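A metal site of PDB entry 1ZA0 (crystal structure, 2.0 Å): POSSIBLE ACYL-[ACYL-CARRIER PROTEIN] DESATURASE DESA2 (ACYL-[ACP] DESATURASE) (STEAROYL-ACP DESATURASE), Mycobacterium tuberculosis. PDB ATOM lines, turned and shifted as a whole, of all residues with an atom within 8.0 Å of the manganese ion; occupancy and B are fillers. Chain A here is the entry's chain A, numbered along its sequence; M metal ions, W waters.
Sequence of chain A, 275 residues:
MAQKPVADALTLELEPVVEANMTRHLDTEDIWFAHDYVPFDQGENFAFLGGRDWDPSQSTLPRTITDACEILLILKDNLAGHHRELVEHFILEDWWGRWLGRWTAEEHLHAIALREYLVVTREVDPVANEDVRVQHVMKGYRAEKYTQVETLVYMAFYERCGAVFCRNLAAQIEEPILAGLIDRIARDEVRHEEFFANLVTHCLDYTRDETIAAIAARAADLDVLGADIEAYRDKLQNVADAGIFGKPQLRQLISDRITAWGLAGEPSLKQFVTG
The side-chain carboxylate (OE1) of Glu 106 sits at hydrogen-bond distance from a ring nitrogen (NE2) of His 192 (2.4 Å).
The side-chain carboxylate (OE1) of Glu 189 is in salt-bridge range of the side-chain amino group (NZ) of Lys 76.
A ring nitrogen (ND1) of His 192 lies close to the indole nitrogen of Trp 103, 3.3 Å away.
The side-chain carboxylate (OE1) of Glu 107 lies within salt-bridge range of the side-chain amino group (NZ) of Lys 76 (3.0 Å).
NZ of Lys 76 is in hydrogen-bond range of ND1 of His 110 (2.9 Å).
The indole nitrogen (NE1) of Trp 103 sits close to the side-chain carboxylate (OE2) of Glu 159 (2.7 Å).
Merely in contact with the manganese ion: Lys 76 (3.8 Å) and Trp 103 (3.9 Å).
Of the 22 residues printed, 6 come within 4 Å of the manganese ion.
The nearest printed residue that does not touch the manganese ion is His 110 (4.8 Å).
The manganese ion is bound by OE2 of Glu 189 (2.1 Å).
The side-chain carboxylate (OE2) of Glu 107 is bound to the manganese ion, at 2.1 Å.
The manganese ion is bound by water W1 (2.2 Å).
OE1 of Glu 159 is bound to the manganese ion (2.3 Å).
ND1 of His 192 is bound to the manganese ion (2.3 Å).
OE2 of Glu 159 binds the manganese ion (2.4 Å).
Water W1 lies within hydrogen-bond range of OE1 of Glu 189 (3.0 Å), OE1 of Glu 107 (3.1 Å) and NZ of Lys 76 (3.4 Å).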
ATOM      1  N   LYS A  76     -20.291  33.179 -23.067  1.00  0.00           N
ATOM      2  CA  LYS A  76     -20.874  33.953 -24.165  1.00  0.00           C
ATOM      3  C   LYS A  76     -19.819  34.837 -24.867  1.00  0.00           C
ATOM      4  O   LYS A  76     -19.904  35.037 -26.055  1.00  0.00           O
ATOM      5  CB  LYS A  76     -22.051  34.817 -23.714  1.00  0.00           C
ATOM      6  CG  LYS A  76     -23.281  34.024 -23.204  1.00  0.00           C
ATOM      7  CD  LYS A  76     -24.197  33.602 -24.232  1.00  0.00           C
ATOM      8  CE  LYS A  76     -25.382  32.813 -23.597  1.00  0.00           C
ATOM      9  NZ  LYS A  76     -26.056  32.308 -24.790  1.00  0.00           N
ATOM     10  N   TRP A  99     -27.757  32.048 -41.149  1.00  0.00           N
ATOM     11  CA  TRP A  99     -27.976  31.535 -39.791  1.00  0.00           C
ATOM     12  C   TRP A  99     -26.786  31.822 -38.890  1.00  0.00           C
ATOM     13  O   TRP A  99     -27.017  32.350 -37.787  1.00  0.00           O
ATOM     14  CB  TRP A  99     -28.321  30.066 -39.770  1.00  0.00           C
ATOM     15  CG  TRP A  99     -28.305  29.422 -38.392  1.00  0.00           C
ATOM     16  CD1 TRP A  99     -27.538  28.370 -38.005  1.00  0.00           C
ATOM     17  CD2 TRP A  99     -29.044  29.806 -37.225  1.00  0.00           C
ATOM     18  NE1 TRP A  99     -27.803  28.028 -36.703  1.00  0.00           N
ATOM     19  CE2 TRP A  99     -28.717  28.886 -36.195  1.00  0.00           C
ATOM     20  CE3 TRP A  99     -29.992  30.792 -36.951  1.00  0.00           C
ATOM     21  CZ2 TRP A  99     -29.258  28.942 -34.898  1.00  0.00           C
ATOM     22  CZ3 TRP A  99     -30.553  30.828 -35.637  1.00  0.00           C
ATOM     23  CH2 TRP A  99     -30.158  29.942 -34.645  1.00  0.00           C
ATOM     24  N   TRP A 103     -27.217  33.770 -35.429  1.00  0.00           N
ATOM     25  CA  TRP A 103     -26.932  33.065 -34.189  1.00  0.00           C
ATOM     26  C   TRP A 103     -25.835  33.821 -33.443  1.00  0.00           C
ATOM     27  O   TRP A 103     -25.974  34.105 -32.259  1.00  0.00           O
ATOM     28  CB  TRP A 103     -26.510  31.606 -34.438  1.00  0.00           C
ATOM     29  CG  TRP A 103     -26.049  30.882 -33.190  1.00  0.00           C
ATOM     30  CD1 TRP A 103     -26.861  30.337 -32.273  1.00  0.00           C
ATOM     31  CD2 TRP A 103     -24.709  30.623 -32.739  1.00  0.00           C
ATOM     32  NE1 TRP A 103     -26.127  29.802 -31.246  1.00  0.00           N
ATOM     33  CE2 TRP A 103     -24.797  29.963 -31.521  1.00  0.00           C
ATOM     34  CE3 TRP A 103     -23.435  30.945 -33.231  1.00  0.00           C
ATOM     35  CZ2 TRP A 103     -23.683  29.590 -30.777  1.00  0.00           C
ATOM     36  CZ3 TRP A 103     -22.332  30.604 -32.491  1.00  0.00           C
ATOM     37  CH2 TRP A 103     -22.451  29.896 -31.289  1.00  0.00           C
ATOM     38  N   GLU A 106     -27.073  36.987 -31.799  1.00  0.00           N
ATOM     39  CA  GLU A 106     -27.873  36.688 -30.591  1.00  0.00           C
ATOM     40  C   GLU A 106     -26.999  36.351 -29.379  1.00  0.00           C
ATOM     41  O   GLU A 106     -27.239  36.885 -28.302  1.00  0.00           O
ATOM     42  CB  GLU A 106     -28.902  35.633 -30.842  1.00  0.00           C
ATOM     43  CG  GLU A 106     -29.974  36.096 -31.825  1.00  0.00           C
ATOM     44  CD  GLU A 106     -31.096  35.027 -32.092  1.00  0.00           C
ATOM     45  OE1 GLU A 106     -31.139  33.935 -31.450  1.00  0.00           O
ATOM     46  OE2 GLU A 106     -31.966  35.358 -32.897  1.00  0.00           O
ATOM     47  N   GLU A 107     -25.987  35.535 -29.587  1.00  0.00           N
ATOM     48  CA  GLU A 107     -25.052  35.203 -28.566  1.00  0.00           C
ATOM     49  C   GLU A 107     -24.346  36.499 -28.042  1.00  0.00           C
ATOM     50  O   GLU A 107     -24.117  36.682 -26.802  1.00  0.00           O
ATOM     51  CB  GLU A 107     -23.991  34.225 -29.081  1.00  0.00           C
ATOM     52  CG  GLU A 107     -24.470  32.816 -29.430  1.00  0.00           C
ATOM     53  CD  GLU A 107     -25.006  32.066 -28.218  1.00  0.00           C
ATOM     54  OE1 GLU A 107     -24.335  31.960 -27.205  1.00  0.00           O
ATOM     55  OE2 GLU A 107     -26.131  31.648 -28.246  1.00  0.00           O
ATOM     56  N   HIS A 110     -26.528  38.596 -25.746  1.00  0.00           N
ATOM     57  CA  HIS A 110     -26.602  38.026 -24.432  1.00  0.00           C
ATOM     58  C   HIS A 110     -25.416  38.507 -23.604  1.00  0.00           C
ATOM     59  O   HIS A 110     -25.619  38.954 -22.463  1.00  0.00           O
ATOM     60  CB  HIS A 110     -26.542  36.443 -24.488  1.00  0.00           C
ATOM     61  CG  HIS A 110     -27.687  35.835 -25.247  1.00  0.00           C
ATOM     62  ND1 HIS A 110     -27.684  34.524 -25.709  1.00  0.00           N
ATOM     63  CD2 HIS A 110     -28.898  36.361 -25.576  1.00  0.00           C
ATOM     64  CE1 HIS A 110     -28.856  34.292 -26.292  1.00  0.00           C
ATOM     65  NE2 HIS A 110     -29.608  35.386 -26.224  1.00  0.00           N
ATOM     66  N   MET A 155     -23.262  21.314 -30.932  1.00  0.00           N
ATOM     67  CA  MET A 155     -24.023  22.501 -30.752  1.00  0.00           C
ATOM     68  C   MET A 155     -25.451  22.239 -30.250  1.00  0.00           C
ATOM     69  O   MET A 155     -25.957  23.010 -29.426  1.00  0.00           O
ATOM     70  CB  MET A 155     -24.083  23.298 -32.036  1.00  0.00           C
ATOM     71  CG  MET A 155     -22.783  23.929 -32.458  1.00  0.00           C
ATOM     72  SD  MET A 155     -22.013  24.961 -31.182  1.00  0.00           S
ATOM     73  CE  MET A 155     -23.332  26.261 -31.086  1.00  0.00           C
ATOM     74  N   TYR A 158     -25.017  21.515 -26.536  1.00  0.00           N
ATOM     75  CA  TYR A 158     -24.461  22.659 -25.858  1.00  0.00           C
ATOM     76  C   TYR A 158     -25.536  23.758 -25.701  1.00  0.00           C
ATOM     77  O   TYR A 158     -25.690  24.310 -24.621  1.00  0.00           O
ATOM     78  CB  TYR A 158     -23.216  23.177 -26.622  1.00  0.00           C
ATOM     79  CG  TYR A 158     -22.582  24.424 -25.999  1.00  0.00           C
ATOM     80  CD1 TYR A 158     -21.716  24.291 -24.918  1.00  0.00           C
ATOM     81  CD2 TYR A 158     -22.879  25.692 -26.441  1.00  0.00           C
ATOM     82  CE1 TYR A 158     -21.116  25.389 -24.313  1.00  0.00           C
ATOM     83  CE2 TYR A 158     -22.281  26.828 -25.842  1.00  0.00           C
ATOM     84  CZ  TYR A 158     -21.421  26.652 -24.753  1.00  0.00           C
ATOM     85  OH  TYR A 158     -20.792  27.718 -24.121  1.00  0.00           O
ATOM     86  N   GLU A 159     -26.325  24.002 -26.744  1.00  0.00           N
ATOM     87  CA  GLU A 159     -27.468  24.854 -26.634  1.00  0.00           C
ATOM     88  C   GLU A 159     -28.529  24.334 -25.682  1.00  0.00           C
ATOM     89  O   GLU A 159     -29.150  25.112 -24.984  1.00  0.00           O
ATOM     90  CB  GLU A 159     -28.087  25.198 -27.992  1.00  0.00           C
ATOM     91  CG  GLU A 159     -27.128  25.981 -28.870  1.00  0.00           C
ATOM     92  CD  GLU A 159     -27.052  27.437 -28.362  1.00  0.00           C
ATOM     93  OE1 GLU A 159     -27.695  27.750 -27.295  1.00  0.00           O
ATOM     94  OE2 GLU A 159     -26.455  28.274 -29.024  1.00  0.00           O
ATOM     95  N   ARG A 160     -28.717  23.026 -25.600  1.00  0.00           N
ATOM     96  CA  ARG A 160     -29.668  22.511 -24.648  1.00  0.00           C
ATOM     97  C   ARG A 160     -29.156  22.749 -23.210  1.00  0.00           C
ATOM     98  O   ARG A 160     -29.918  23.085 -22.365  1.00  0.00           O
ATOM     99  CB  ARG A 160     -29.927  21.020 -24.859  1.00  0.00           C
ATOM    100  CG  ARG A 160     -31.056  20.465 -23.945  1.00  0.00           C
ATOM    101  CD  ARG A 160     -31.493  19.056 -24.332  1.00  0.00           C
ATOM    102  NE  ARG A 160     -32.753  18.660 -23.709  1.00  0.00           N
ATOM    103  CZ  ARG A 160     -33.948  18.607 -24.261  1.00  0.00           C
ATOM    104  NH1 ARG A 160     -34.152  18.955 -25.515  1.00  0.00           N
ATOM    105  NH2 ARG A 160     -34.969  18.205 -23.518  1.00  0.00           N
ATOM    106  N   GLY A 162     -27.274  25.273 -22.306  1.00  0.00           N
ATOM    107  CA  GLY A 162     -27.612  26.704 -22.188  1.00  0.00           C
ATOM    108  C   GLY A 162     -29.052  26.936 -21.787  1.00  0.00           C
ATOM    109  O   GLY A 162     -29.328  27.777 -20.920  1.00  0.00           O
ATOM    110  N   ALA A 163     -29.975  26.222 -22.430  1.00  0.00           N
ATOM    111  CA  ALA A 163     -31.389  26.423 -22.210  1.00  0.00           C
ATOM    112  C   ALA A 163     -31.821  25.959 -20.800  1.00  0.00           C
ATOM    113  O   ALA A 163     -32.545  26.712 -20.148  1.00  0.00           O
ATOM    114  CB  ALA A 163     -32.197  25.723 -23.271  1.00  0.00           C
ATOM    115  N   CYS A 166     -30.159  28.439 -18.123  1.00  0.00           N
ATOM    116  CA  CYS A 166     -30.752  29.735 -18.023  1.00  0.00           C
ATOM    117  C   CYS A 166     -32.209  29.667 -17.530  1.00  0.00           C
ATOM    118  O   CYS A 166     -32.684  30.574 -16.814  1.00  0.00           O
ATOM    119  CB  CYS A 166     -30.694  30.477 -19.356  1.00  0.00           C
ATOM    120  SG  CYS A 166     -29.021  30.904 -19.843  1.00  0.00           S
ATOM    121  N   ILE A 185     -32.834  35.454 -22.501  1.00  0.00           N
ATOM    122  CA  ILE A 185     -31.721  34.603 -22.910  1.00  0.00           C
ATOM    123  C   ILE A 185     -32.132  33.126 -23.014  1.00  0.00           C
ATOM    124  O   ILE A 185     -31.829  32.429 -24.048  1.00  0.00           O
ATOM    125  CB  ILE A 185     -30.526  34.740 -21.957  1.00  0.00           C
ATOM    126  CG1 ILE A 185     -29.939  36.154 -22.033  1.00  0.00           C
ATOM    127  CG2 ILE A 185     -29.439  33.708 -22.271  1.00  0.00           C
ATOM    128  CD1 ILE A 185     -28.704  36.341 -21.074  1.00  0.00           C
ATOM    129  N   ALA A 186     -32.862  32.651 -21.986  1.00  0.00           N
ATOM    130  CA  ALA A 186     -33.329  31.266 -21.961  1.00  0.00           C
ATOM    131  C   ALA A 186     -34.185  30.949 -23.201  1.00  0.00           C
ATOM    132  O   ALA A 186     -34.025  29.857 -23.780  1.00  0.00           O
ATOM    133  CB  ALA A 186     -34.101  30.964 -20.749  1.00  0.00           C
ATOM    134  N   ASP A 188     -34.130  32.452 -26.135  1.00  0.00           N
ATOM    135  CA  ASP A 188     -33.233  32.391 -27.276  1.00  0.00           C
ATOM    136  C   ASP A 188     -32.527  31.059 -27.304  1.00  0.00           C
ATOM    137  O   ASP A 188     -32.439  30.464 -28.363  1.00  0.00           O
ATOM    138  CB  ASP A 188     -32.197  33.528 -27.279  1.00  0.00           C
ATOM    139  CG  ASP A 188     -32.768  34.869 -27.632  1.00  0.00           C
ATOM    140  OD1 ASP A 188     -33.865  35.003 -28.273  1.00  0.00           O
ATOM    141  OD2 ASP A 188     -32.140  35.909 -27.317  1.00  0.00           O
ATOM    142  N   GLU A 189     -32.077  30.550 -26.158  1.00  0.00           N
ATOM    143  CA  GLU A 189     -31.368  29.314 -26.138  1.00  0.00           C
ATOM    144  C   GLU A 189     -32.273  28.107 -26.582  1.00  0.00           C
ATOM    145  O   GLU A 189     -31.765  27.185 -27.244  1.00  0.00           O
ATOM    146  CB  GLU A 189     -30.781  28.984 -24.757  1.00  0.00           C
ATOM    147  CG  GLU A 189     -29.894  30.066 -24.154  1.00  0.00           C
ATOM    148  CD  GLU A 189     -28.542  30.214 -24.835  1.00  0.00           C
ATOM    149  OE1 GLU A 189     -27.496  30.031 -24.126  1.00  0.00           O
ATOM    150  OE2 GLU A 189     -28.520  30.589 -26.040  1.00  0.00           O
ATOM    151  N   VAL A 190     -33.556  28.158 -26.238  1.00  0.00           N
ATOM    152  CA  VAL A 190     -34.515  27.157 -26.709  1.00  0.00           C
ATOM    153  C   VAL A 190     -34.584  27.142 -28.252  1.00  0.00           C
ATOM    154  O   VAL A 190     -34.596  26.079 -28.908  1.00  0.00           O
ATOM    155  CB  VAL A 190     -35.891  27.354 -26.024  1.00  0.00           C
ATOM    156  CG1 VAL A 190     -37.024  26.566 -26.749  1.00  0.00           C
ATOM    157  CG2 VAL A 190     -35.810  26.997 -24.519  1.00  0.00           C
ATOM    158  N   ARG A 191     -34.627  28.329 -28.792  1.00  0.00           N
ATOM    159  CA  ARG A 191     -34.626  28.556 -30.221  1.00  0.00           C
ATOM    160  C   ARG A 191     -33.347  28.115 -30.903  1.00  0.00           C
ATOM    161  O   ARG A 191     -33.392  27.506 -31.995  1.00  0.00           O
ATOM    162  CB  ARG A 191     -34.978  30.004 -30.527  1.00  0.00           C
ATOM    163  CG  ARG A 191     -36.394  30.312 -30.231  1.00  0.00           C
ATOM    164  CD  ARG A 191     -36.702  31.811 -30.160  1.00  0.00           C
ATOM    165  NE  ARG A 191     -36.327  32.604 -31.333  1.00  0.00           N
ATOM    166  CZ  ARG A 191     -37.089  32.729 -32.432  1.00  0.00           C
ATOM    167  NH1 ARG A 191     -38.203  32.027 -32.568  1.00  0.00           N
ATOM    168  NH2 ARG A 191     -36.721  33.523 -33.432  1.00  0.00           N
ATOM    169  N   HIS A 192     -32.193  28.308 -30.230  1.00  0.00           N
ATOM    170  CA  HIS A 192     -30.931  27.896 -30.751  1.00  0.00           C
ATOM    171  C   HIS A 192     -30.880  26.357 -30.816  1.00  0.00           C
ATOM    172  O   HIS A 192     -30.429  25.719 -31.834  1.00  0.00           O
ATOM    173  CB  HIS A 192     -29.783  28.490 -29.888  1.00  0.00           C
ATOM    174  CG  HIS A 192     -29.638  29.994 -29.981  1.00  0.00           C
ATOM    175  ND1 HIS A 192     -28.666  30.701 -29.296  1.00  0.00           N
ATOM    176  CD2 HIS A 192     -30.402  30.924 -30.633  1.00  0.00           C
ATOM    177  CE1 HIS A 192     -28.781  31.992 -29.605  1.00  0.00           C
ATOM    178  NE2 HIS A 192     -29.840  32.164 -30.366  1.00  0.00           N
ATOM    179  N   GLU A 193     -31.253  25.753 -29.711  1.00  0.00           N
ATOM    180  CA  GLU A 193     -31.251  24.337 -29.626  1.00  0.00           C
ATOM    181  C   GLU A 193     -32.167  23.703 -30.739  1.00  0.00           C
ATOM    182  O   GLU A 193     -31.801  22.674 -31.308  1.00  0.00           O
ATOM    183  CB  GLU A 193     -31.628  23.830 -28.224  1.00  0.00           C
ATOM    184  CG  GLU A 193     -31.515  22.295 -28.140  1.00  0.00           C
ATOM    185  CD  GLU A 193     -32.417  21.627 -27.107  1.00  0.00           C
ATOM    186  OE1 GLU A 193     -33.095  22.351 -26.316  1.00  0.00           O
ATOM    187  OE2 GLU A 193     -32.410  20.354 -27.048  1.00  0.00           O
ATOM    188  N   PHE A 196     -30.374  23.907 -34.209  1.00  0.00           N
ATOM    189  CA  PHE A 196     -29.331  22.906 -34.367  1.00  0.00           C
ATOM    190  C   PHE A 196     -29.884  21.508 -34.314  1.00  0.00           C
ATOM    191  O   PHE A 196     -29.435  20.600 -35.044  1.00  0.00           O
ATOM    192  CB  PHE A 196     -28.159  23.063 -33.392  1.00  0.00           C
ATOM    193  CG  PHE A 196     -27.328  24.294 -33.668  1.00  0.00           C
ATOM    194  CD1 PHE A 196     -26.544  24.369 -34.826  1.00  0.00           C
ATOM    195  CD2 PHE A 196     -27.343  25.363 -32.799  1.00  0.00           C
ATOM    196  CE1 PHE A 196     -25.775  25.500 -35.088  1.00  0.00           C
ATOM    197  CE2 PHE A 196     -26.567  26.504 -33.054  1.00  0.00           C
ATOM    198  CZ  PHE A 196     -25.820  26.576 -34.215  1.00  0.00           C
HETATM  199 MN    MN M   1     -27.262  29.967 -27.566  1.00  0.00          MN
HETATM  200  O   HOH W   1     -25.603  29.325 -26.325  1.00  0.00           O
